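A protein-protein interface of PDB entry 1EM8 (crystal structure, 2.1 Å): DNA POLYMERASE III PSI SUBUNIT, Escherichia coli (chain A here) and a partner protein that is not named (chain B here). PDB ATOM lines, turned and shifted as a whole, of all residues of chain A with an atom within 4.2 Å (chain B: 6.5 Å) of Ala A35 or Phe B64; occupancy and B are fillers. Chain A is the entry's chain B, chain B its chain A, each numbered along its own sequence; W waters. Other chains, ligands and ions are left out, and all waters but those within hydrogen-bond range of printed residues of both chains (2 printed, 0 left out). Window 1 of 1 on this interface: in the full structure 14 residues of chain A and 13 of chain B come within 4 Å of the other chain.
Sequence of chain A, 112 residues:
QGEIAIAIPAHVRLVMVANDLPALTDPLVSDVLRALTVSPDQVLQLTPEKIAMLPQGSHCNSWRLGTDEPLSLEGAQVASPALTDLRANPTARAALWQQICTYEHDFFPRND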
ATOM      1  N   LEU A  28     -21.696  25.381  17.684  1.00  0.00           N
ATOM      2  CA  LEU A  28     -20.700  24.724  16.858  1.00  0.00           C
ATOM      3  C   LEU A  28     -19.417  25.547  16.740  1.00  0.00           C
ATOM      4  O   LEU A  28     -18.322  24.997  16.881  1.00  0.00           O
ATOM      5  CB  LEU A  28     -21.281  24.432  15.473  1.00  0.00           C
ATOM      6  CG  LEU A  28     -20.320  23.770  14.487  1.00  0.00           C
ATOM      7  CD1 LEU A  28     -19.792  22.478  15.086  1.00  0.00           C
ATOM      8  CD2 LEU A  28     -21.036  23.510  13.166  1.00  0.00           C
ATOM      9  N   ASP A  31     -17.310  25.307  19.897  1.00  0.00           N
ATOM     10  CA  ASP A  31     -16.595  24.045  20.070  1.00  0.00           C
ATOM     11  C   ASP A  31     -15.363  23.989  19.153  1.00  0.00           C
ATOM     12  O   ASP A  31     -14.328  23.444  19.528  1.00  0.00           O
ATOM     13  CB  ASP A  31     -17.508  22.846  19.778  1.00  0.00           C
ATOM     14  CG  ASP A  31     -18.417  22.487  20.950  1.00  0.00           C
ATOM     15  OD1 ASP A  31     -18.280  23.072  22.044  1.00  0.00           O
ATOM     16  OD2 ASP A  31     -19.266  21.581  20.772  1.00  0.00           O
ATOM     17  N   VAL A  32     -15.476  24.537  17.947  1.00  0.00           N
ATOM     18  CA  VAL A  32     -14.341  24.520  17.032  1.00  0.00           C
ATOM     19  C   VAL A  32     -13.223  25.407  17.576  1.00  0.00           C
ATOM     20  O   VAL A  32     -12.045  25.073  17.464  1.00  0.00           O
ATOM     21  CB  VAL A  32     -14.736  25.003  15.616  1.00  0.00           C
ATOM     22  CG1 VAL A  32     -13.500  25.063  14.722  1.00  0.00           C
ATOM     23  CG2 VAL A  32     -15.765  24.051  15.013  1.00  0.00           C
ATOM     24  N   LEU A  33     -13.594  26.536  18.165  1.00  0.00           N
ATOM     25  CA  LEU A  33     -12.598  27.437  18.732  1.00  0.00           C
ATOM     26  C   LEU A  33     -11.887  26.740  19.886  1.00  0.00           C
ATOM     27  O   LEU A  33     -10.662  26.820  20.010  1.00  0.00           O
ATOM     28  CB  LEU A  33     -13.259  28.737  19.201  1.00  0.00           C
ATOM     29  CG  LEU A  33     -13.816  29.585  18.045  1.00  0.00           C
ATOM     30  CD1 LEU A  33     -14.525  30.813  18.587  1.00  0.00           C
ATOM     31  CD2 LEU A  33     -12.683  29.992  17.124  1.00  0.00           C
ATOM     32  N   ARG A  34     -12.649  26.037  20.715  1.00  0.00           N
ATOM     33  CA  ARG A  34     -12.067  25.310  21.835  1.00  0.00           C
ATOM     34  C   ARG A  34     -11.138  24.201  21.320  1.00  0.00           C
ATOM     35  O   ARG A  34     -10.085  23.944  21.899  1.00  0.00           O
ATOM     36  CB  ARG A  34     -13.188  24.740  22.705  1.00  0.00           C
ATOM     37  CG  ARG A  34     -12.751  23.879  23.873  1.00  0.00           C
ATOM     38  CD  ARG A  34     -13.886  23.799  24.892  1.00  0.00           C
ATOM     39  NE  ARG A  34     -13.908  25.008  25.709  1.00  0.00           N
ATOM     40  CZ  ARG A  34     -14.954  25.446  26.397  1.00  0.00           C
ATOM     41  NH1 ARG A  34     -16.099  24.774  26.382  1.00  0.00           N
ATOM     42  NH2 ARG A  34     -14.851  26.561  27.106  1.00  0.00           N
ATOM     43  N   ALA A  35     -11.525  23.565  20.221  1.00  0.00           N
ATOM     44  CA  ALA A  35     -10.718  22.507  19.612  1.00  0.00           C
ATOM     45  C   ALA A  35      -9.375  23.100  19.188  1.00  0.00           C
ATOM     46  O   ALA A  35      -8.336  22.456  19.307  1.00  0.00           O
ATOM     47  CB  ALA A  35     -11.441  21.927  18.388  1.00  0.00           C
ATOM     48  N   LEU A  36      -9.420  24.331  18.677  1.00  0.00           N
ATOM     49  CA  LEU A  36      -8.229  25.047  18.234  1.00  0.00           C
ATOM     50  C   LEU A  36      -7.491  25.734  19.388  1.00  0.00           C
ATOM     51  O   LEU A  36      -6.526  26.452  19.160  1.00  0.00           O
ATOM     52  CB  LEU A  36      -8.612  26.115  17.201  1.00  0.00           C
ATOM     53  CG  LEU A  36      -9.239  25.662  15.882  1.00  0.00           C
ATOM     54  CD1 LEU A  36      -9.855  26.866  15.175  1.00  0.00           C
ATOM     55  CD2 LEU A  36      -8.170  24.993  15.006  1.00  0.00           C
ATOM     56  N   THR A  37      -7.950  25.496  20.620  1.00  0.00           N
ATOM     57  CA  THR A  37      -7.386  26.138  21.794  1.00  0.00           C
ATOM     58  C   THR A  37      -7.270  27.636  21.579  1.00  0.00           C
ATOM     59  O   THR A  37      -6.284  28.278  21.911  1.00  0.00           O
ATOM     60  CB  THR A  37      -6.017  25.558  22.149  1.00  0.00           C
ATOM     61  OG1 THR A  37      -5.027  26.083  21.257  1.00  0.00           O
ATOM     62  CG2 THR A  37      -6.044  24.040  22.050  1.00  0.00           C
ATOM     63  N   ARG A  93     -17.178  17.503   9.786  1.00  0.00           N
ATOM     64  CA  ARG A  93     -16.588  17.858  11.068  1.00  0.00           C
ATOM     65  C   ARG A  93     -15.343  17.017  11.348  1.00  0.00           C
ATOM     66  O   ARG A  93     -14.318  17.526  11.801  1.00  0.00           O
ATOM     67  CB  ARG A  93     -17.615  17.690  12.195  1.00  0.00           C
ATOM     68  CG  ARG A  93     -18.807  18.642  12.093  1.00  0.00           C
ATOM     69  CD  ARG A  93     -19.591  18.716  13.402  1.00  0.00           C
ATOM     70  NE  ARG A  93     -20.487  17.589  13.632  1.00  0.00           N
ATOM     71  CZ  ARG A  93     -21.633  17.400  12.980  1.00  0.00           C
ATOM     72  NH1 ARG A  93     -22.022  18.260  12.048  1.00  0.00           N
ATOM     73  NH2 ARG A  93     -22.396  16.355  13.264  1.00  0.00           N
ATOM     74  N   LEU A  96     -12.623  18.352   9.280  1.00  0.00           N
ATOM     75  CA  LEU A  96     -12.090  19.612   9.789  1.00  0.00           C
ATOM     76  C   LEU A  96     -11.054  19.292  10.877  1.00  0.00           C
ATOM     77  O   LEU A  96      -9.955  19.852  10.871  1.00  0.00           O
ATOM     78  CB  LEU A  96     -13.208  20.482  10.377  1.00  0.00           C
ATOM     79  CG  LEU A  96     -13.023  22.010  10.344  1.00  0.00           C
ATOM     80  CD1 LEU A  96     -14.228  22.665  11.011  1.00  0.00           C
ATOM     81  CD2 LEU A  96     -11.765  22.442  11.048  1.00  0.00           C
ATOM     82  N   TRP A  97     -11.400  18.392  11.802  1.00  0.00           N
ATOM     83  CA  TRP A  97     -10.482  18.006  12.883  1.00  0.00           C
ATOM     84  C   TRP A  97      -9.188  17.441  12.309  1.00  0.00           C
ATOM     85  O   TRP A  97      -8.092  17.787  12.754  1.00  0.00           O
ATOM     86  CB  TRP A  97     -11.110  16.944  13.795  1.00  0.00           C
ATOM     87  CG  TRP A  97     -10.181  16.453  14.892  1.00  0.00           C
ATOM     88  CD1 TRP A  97      -9.822  15.159  15.141  1.00  0.00           C
ATOM     89  CD2 TRP A  97      -9.500  17.249  15.885  1.00  0.00           C
ATOM     90  NE1 TRP A  97      -8.961  15.096  16.215  1.00  0.00           N
ATOM     91  CE2 TRP A  97      -8.754  16.363  16.693  1.00  0.00           C
ATOM     92  CE3 TRP A  97      -9.462  18.620  16.170  1.00  0.00           C
ATOM     93  CZ2 TRP A  97      -7.964  16.805  17.763  1.00  0.00           C
ATOM     94  CZ3 TRP A  97      -8.676  19.062  17.236  1.00  0.00           C
ATOM     95  CH2 TRP A  97      -7.938  18.154  18.018  1.00  0.00           C
ATOM     96  N   PHE A 108      -1.408  23.642  18.508  1.00  0.00           N
ATOM     97  CA  PHE A 108      -1.101  23.005  19.802  1.00  0.00           C
ATOM     98  C   PHE A 108       0.412  22.918  19.993  1.00  0.00           C
ATOM     99  O   PHE A 108       0.956  21.824  20.162  1.00  0.00           O
ATOM    100  CB  PHE A 108      -1.645  21.571  19.852  1.00  0.00           C
ATOM    101  CG  PHE A 108      -3.006  21.405  19.244  1.00  0.00           C
ATOM    102  CD1 PHE A 108      -3.268  20.321  18.414  1.00  0.00           C
ATOM    103  CD2 PHE A 108      -4.009  22.338  19.467  1.00  0.00           C
ATOM    104  CE1 PHE A 108      -4.516  20.163  17.817  1.00  0.00           C
ATOM    105  CE2 PHE A 108      -5.256  22.189  18.877  1.00  0.00           C
ATOM    106  CZ  PHE A 108      -5.510  21.101  18.045  1.00  0.00           C
ATOM    107  N   TRP B  33     -15.203  17.339  28.302  1.00  0.00           N
ATOM    108  CA  TRP B  33     -14.213  17.999  27.462  1.00  0.00           C
ATOM    109  C   TRP B  33     -14.450  19.504  27.460  1.00  0.00           C
ATOM    110  O   TRP B  33     -13.525  20.298  27.633  1.00  0.00           O
ATOM    111  CB  TRP B  33     -14.312  17.515  26.019  1.00  0.00           C
ATOM    112  CG  TRP B  33     -13.566  18.400  25.072  1.00  0.00           C
ATOM    113  CD1 TRP B  33     -12.208  18.530  24.956  1.00  0.00           C
ATOM    114  CD2 TRP B  33     -14.140  19.328  24.135  1.00  0.00           C
ATOM    115  NE1 TRP B  33     -11.906  19.473  23.997  1.00  0.00           N
ATOM    116  CE2 TRP B  33     -13.073  19.976  23.483  1.00  0.00           C
ATOM    117  CE3 TRP B  33     -15.455  19.661  23.784  1.00  0.00           C
ATOM    118  CZ2 TRP B  33     -13.279  20.948  22.497  1.00  0.00           C
ATOM    119  CZ3 TRP B  33     -15.661  20.632  22.800  1.00  0.00           C
ATOM    120  CH2 TRP B  33     -14.576  21.260  22.169  1.00  0.00           C
ATOM    121  N   ARG B  34     -15.708  19.879  27.266  1.00  0.00           N
ATOM    122  CA  ARG B  34     -16.090  21.278  27.201  1.00  0.00           C
ATOM    123  C   ARG B  34     -15.764  21.994  28.515  1.00  0.00           C
ATOM    124  O   ARG B  34     -15.519  23.196  28.526  1.00  0.00           O
ATOM    125  CB  ARG B  34     -17.581  21.365  26.855  1.00  0.00           C
ATOM    126  CG  ARG B  34     -18.085  22.736  26.444  1.00  0.00           C
ATOM    127  CD  ARG B  34     -19.497  22.606  25.909  1.00  0.00           C
ATOM    128  NE  ARG B  34     -19.551  21.922  24.615  1.00  0.00           N
ATOM    129  CZ  ARG B  34     -20.453  20.999  24.296  1.00  0.00           C
ATOM    130  NH1 ARG B  34     -21.367  20.640  25.185  1.00  0.00           N
ATOM    131  NH2 ARG B  34     -20.472  20.468  23.082  1.00  0.00           N
ATOM    132  N   LEU B  56     -19.282   9.940  18.055  1.00  0.00           N
ATOM    133  CA  LEU B  56     -18.916  11.253  18.588  1.00  0.00           C
ATOM    134  C   LEU B  56     -18.867  12.417  17.599  1.00  0.00           C
ATOM    135  O   LEU B  56     -18.764  13.566  18.014  1.00  0.00           O
ATOM    136  CB  LEU B  56     -17.592  11.175  19.358  1.00  0.00           C
ATOM    137  CG  LEU B  56     -17.751  11.129  20.881  1.00  0.00           C
ATOM    138  CD1 LEU B  56     -16.396  10.978  21.554  1.00  0.00           C
ATOM    139  CD2 LEU B  56     -18.431  12.404  21.344  1.00  0.00           C
ATOM    140  N   TRP B  57     -18.927  12.128  16.300  1.00  0.00           N
ATOM    141  CA  TRP B  57     -18.950  13.194  15.304  1.00  0.00           C
ATOM    142  C   TRP B  57     -20.394  13.581  14.975  1.00  0.00           C
ATOM    143  O   TRP B  57     -20.641  14.619  14.357  1.00  0.00           O
ATOM    144  CB  TRP B  57     -18.221  12.772  14.022  1.00  0.00           C
ATOM    145  CG  TRP B  57     -16.723  12.720  14.161  1.00  0.00           C
ATOM    146  CD1 TRP B  57     -15.916  11.633  13.958  1.00  0.00           C
ATOM    147  CD2 TRP B  57     -15.857  13.798  14.538  1.00  0.00           C
ATOM    148  NE1 TRP B  57     -14.604  11.966  14.204  1.00  0.00           N
ATOM    149  CE2 TRP B  57     -14.538  13.287  14.558  1.00  0.00           C
ATOM    150  CE3 TRP B  57     -16.067  15.142  14.871  1.00  0.00           C
ATOM    151  CZ2 TRP B  57     -13.434  14.075  14.898  1.00  0.00           C
ATOM    152  CZ3 TRP B  57     -14.962  15.931  15.208  1.00  0.00           C
ATOM    153  CH2 TRP B  57     -13.664  15.391  15.221  1.00  0.00           C
ATOM    154  N   PRO B  60     -22.948  14.579  20.875  1.00  0.00           N
ATOM    155  CA  PRO B  60     -24.242  15.272  20.966  1.00  0.00           C
ATOM    156  C   PRO B  60     -24.519  16.135  19.728  1.00  0.00           C
ATOM    157  O   PRO B  60     -23.607  16.457  18.973  1.00  0.00           O
ATOM    158  CB  PRO B  60     -24.081  16.127  22.223  1.00  0.00           C
ATOM    159  CG  PRO B  60     -23.049  15.361  23.030  1.00  0.00           C
ATOM    160  CD  PRO B  60     -22.056  15.066  21.940  1.00  0.00           C
ATOM    161  N   GLU B  62     -25.175  19.305  17.321  1.00  0.00           N
ATOM    162  CA  GLU B  62     -24.566  20.628  17.244  1.00  0.00           C
ATOM    163  C   GLU B  62     -23.301  20.796  18.069  1.00  0.00           C
ATOM    164  O   GLU B  62     -23.120  21.802  18.767  1.00  0.00           O
ATOM    165  CB  GLU B  62     -25.582  21.706  17.637  1.00  0.00           C
ATOM    166  CG  GLU B  62     -26.531  22.083  16.504  1.00  0.00           C
ATOM    167  CD  GLU B  62     -27.392  23.289  16.831  1.00  0.00           C
ATOM    168  OE1 GLU B  62     -28.421  23.126  17.515  1.00  0.00           O
ATOM    169  OE2 GLU B  62     -27.016  24.406  16.416  1.00  0.00           O
ATOM    170  N   SER B  63     -22.414  19.811  17.974  1.00  0.00           N
ATOM    171  CA  SER B  63     -21.169  19.866  18.712  1.00  0.00           C
ATOM    172  C   SER B  63     -19.989  19.461  17.839  1.00  0.00           C
ATOM    173  O   SER B  63     -20.156  18.818  16.797  1.00  0.00           O
ATOM    174  CB  SER B  63     -21.238  18.932  19.914  1.00  0.00           C
ATOM    175  OG  SER B  63     -21.163  17.588  19.485  1.00  0.00           O
ATOM    176  N   PHE B  64     -18.797  19.862  18.264  1.00  0.00           N
ATOM    177  CA  PHE B  64     -17.571  19.510  17.561  1.00  0.00           C
ATOM    178  C   PHE B  64     -16.691  19.031  18.711  1.00  0.00           C
ATOM    179  O   PHE B  64     -16.085  19.841  19.413  1.00  0.00           O
ATOM    180  CB  PHE B  64     -16.949  20.740  16.894  1.00  0.00           C
ATOM    181  CG  PHE B  64     -15.763  20.430  16.016  1.00  0.00           C
ATOM    182  CD1 PHE B  64     -15.946  20.036  14.694  1.00  0.00           C
ATOM    183  CD2 PHE B  64     -14.468  20.529  16.510  1.00  0.00           C
ATOM    184  CE1 PHE B  64     -14.857  19.751  13.876  1.00  0.00           C
ATOM    185  CE2 PHE B  64     -13.369  20.246  15.699  1.00  0.00           C
ATOM    186  CZ  PHE B  64     -13.566  19.857  14.379  1.00  0.00           C
ATOM    187  N   VAL B  65     -16.666  17.720  18.930  1.00  0.00           N
ATOM    188  CA  VAL B  65     -15.874  17.133  20.006  1.00  0.00           C
ATOM    189  C   VAL B  65     -14.623  16.508  19.410  1.00  0.00           C
ATOM    190  O   VAL B  65     -14.670  15.438  18.802  1.00  0.00           O
ATOM    191  CB  VAL B  65     -16.693  16.061  20.791  1.00  0.00           C
ATOM    192  CG1 VAL B  65     -15.869  15.504  21.951  1.00  0.00           C
ATOM    193  CG2 VAL B  65     -17.983  16.683  21.324  1.00  0.00           C
ATOM    194  N   PRO B  66     -13.478  17.186  19.559  1.00  0.00           N
ATOM    195  CA  PRO B  66     -12.205  16.691  19.028  1.00  0.00           C
ATOM    196  C   PRO B  66     -11.826  15.353  19.674  1.00  0.00           C
ATOM    197  O   PRO B  66     -11.598  15.296  20.881  1.00  0.00           O
ATOM    198  CB  PRO B  66     -11.235  17.814  19.383  1.00  0.00           C
ATOM    199  CG  PRO B  66     -11.839  18.347  20.690  1.00  0.00           C
ATOM    200  CD  PRO B  66     -13.274  18.484  20.236  1.00  0.00           C
ATOM    201  N   PRO B  79      -8.043  15.492  22.584  1.00  0.00           N
ATOM    202  CA  PRO B  79      -8.637  15.824  23.880  1.00  0.00           C
ATOM    203  C   PRO B  79      -9.493  14.659  24.392  1.00  0.00           C
ATOM    204  O   PRO B  79      -9.524  14.375  25.592  1.00  0.00           O
ATOM    205  CB  PRO B  79      -9.437  17.092  23.566  1.00  0.00           C
ATOM    206  CG  PRO B  79      -8.584  17.741  22.470  1.00  0.00           C
ATOM    207  CD  PRO B  79      -8.377  16.525  21.585  1.00  0.00           C
HETATM  208  O   HOH W   1      -9.318  20.835  23.297  1.00  0.00           O
HETATM  209  O   HOH W   2     -22.347  22.037  21.338  1.00  0.00           O
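The guanidinium group of Arg B34 is in salt-bridge range of the side-chain carboxylate of Asp A31, at 2.8 Å.
O of Arg B34 is in hydrogen-bond range of NH1 of Arg A34.
O of Trp B57 lies within hydrogen-bond range of NH2 of Arg A93, 2.7 Å away.
The backbone carbonyl oxygen of Ser B63 sits at hydrogen-bond distance from the guanidinium group of Arg A93, 3.4 Å away.
OD2 of Asp A31 is in hydrogen-bond range of N of Phe B64 (3.1 Å).
Water W2 lies within hydrogen-bond range of the backbone carbonyl oxygen of Glu B62 (2.7 Å), the guanidinium group of Arg B34 (3.0 Å) and the side-chain carboxylate of Asp A31 (3.2 Å).
Water W1 lies within hydrogen-bond range of NE1 of Trp B33 and O of Arg A34.
Of the 11 printed residues of chain B, 7 touch a printed residue of chain A.
Hydrophobic or aromatic side chains of chain B that line the printed part of chain A: Trp B33, Trp B57, Phe B64, Pro B66 and Pro B79.
Among the printed residues, Asp or Glu carboxylates within 4 Å of a Lys or Arg side-chain nitrogen of the other chain: Asp A31 with Arg B34.
O of Pro B60 is in hydrogen-bond range of OG of Ser B63, 2.7 Å away.
Phe B64 touches Leu A28.
Asp A31 touches Trp B33 (O to CH2, 3.4 Å).
Asp A31 touches Ser B63.
Phe B64 touches Val A32.
CG of Arg A34 touches CZ2 of Trp B33, 3.3 Å away.
Phe B64 touches Arg A93.
CB of Leu A96 touches CE1 of Phe B64, at 3.9 Å.
Trp A97 touches Trp B57 (CB to CH2, 3.3 Å).
Pro B66 touches Trp A97.
Trp A97 touches Pro B79.
Ala A35 touches just these residues of chain B: Trp B33 (3.9 Å) and Phe B64 (3.7 Å).
Of chain A, only Leu A28 (3.8 Å), Asp A31 (3.1 Å), Val A32 (3.8 Å), Ala A35 (3.7 Å), Arg A93 (3.1 Å), Leu A96 (3.9 Å) and Trp A97 (3.7 Å) come within 4 Å of Phe B64.
Of the printed residues of chain B, Leu A96 touches Phe B64 (3.9 Å).
Of the printed residues of chain A, Ser B63 touches Asp A31 (3.3 Å) and Arg A93 (3.4 Å).
Printed residues of chain A within 4 Å of Pro B79: Trp A97.
Of the printed residues of chain B, Arg A93 touches Trp B57 (2.7 Å), Ser B63 (3.4 Å) and Phe B64 (3.1 Å).
Of the printed residues of chain B, Asp A31 touches Trp B33, Arg B34, Ser B63 and Phe B64.
Leu B56 touches none of the printed residues of chain A.
The nearest residue of chain B that does not touch Ala A35 is Pro B66 (4.2 Å).
The nearest printed residue of chain A that does not touch Phe B64 is Leu A33 (6.3 Å).
The nearest printed residue of chain A that does not touch Arg B34 is Leu A28 (7.4 Å).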
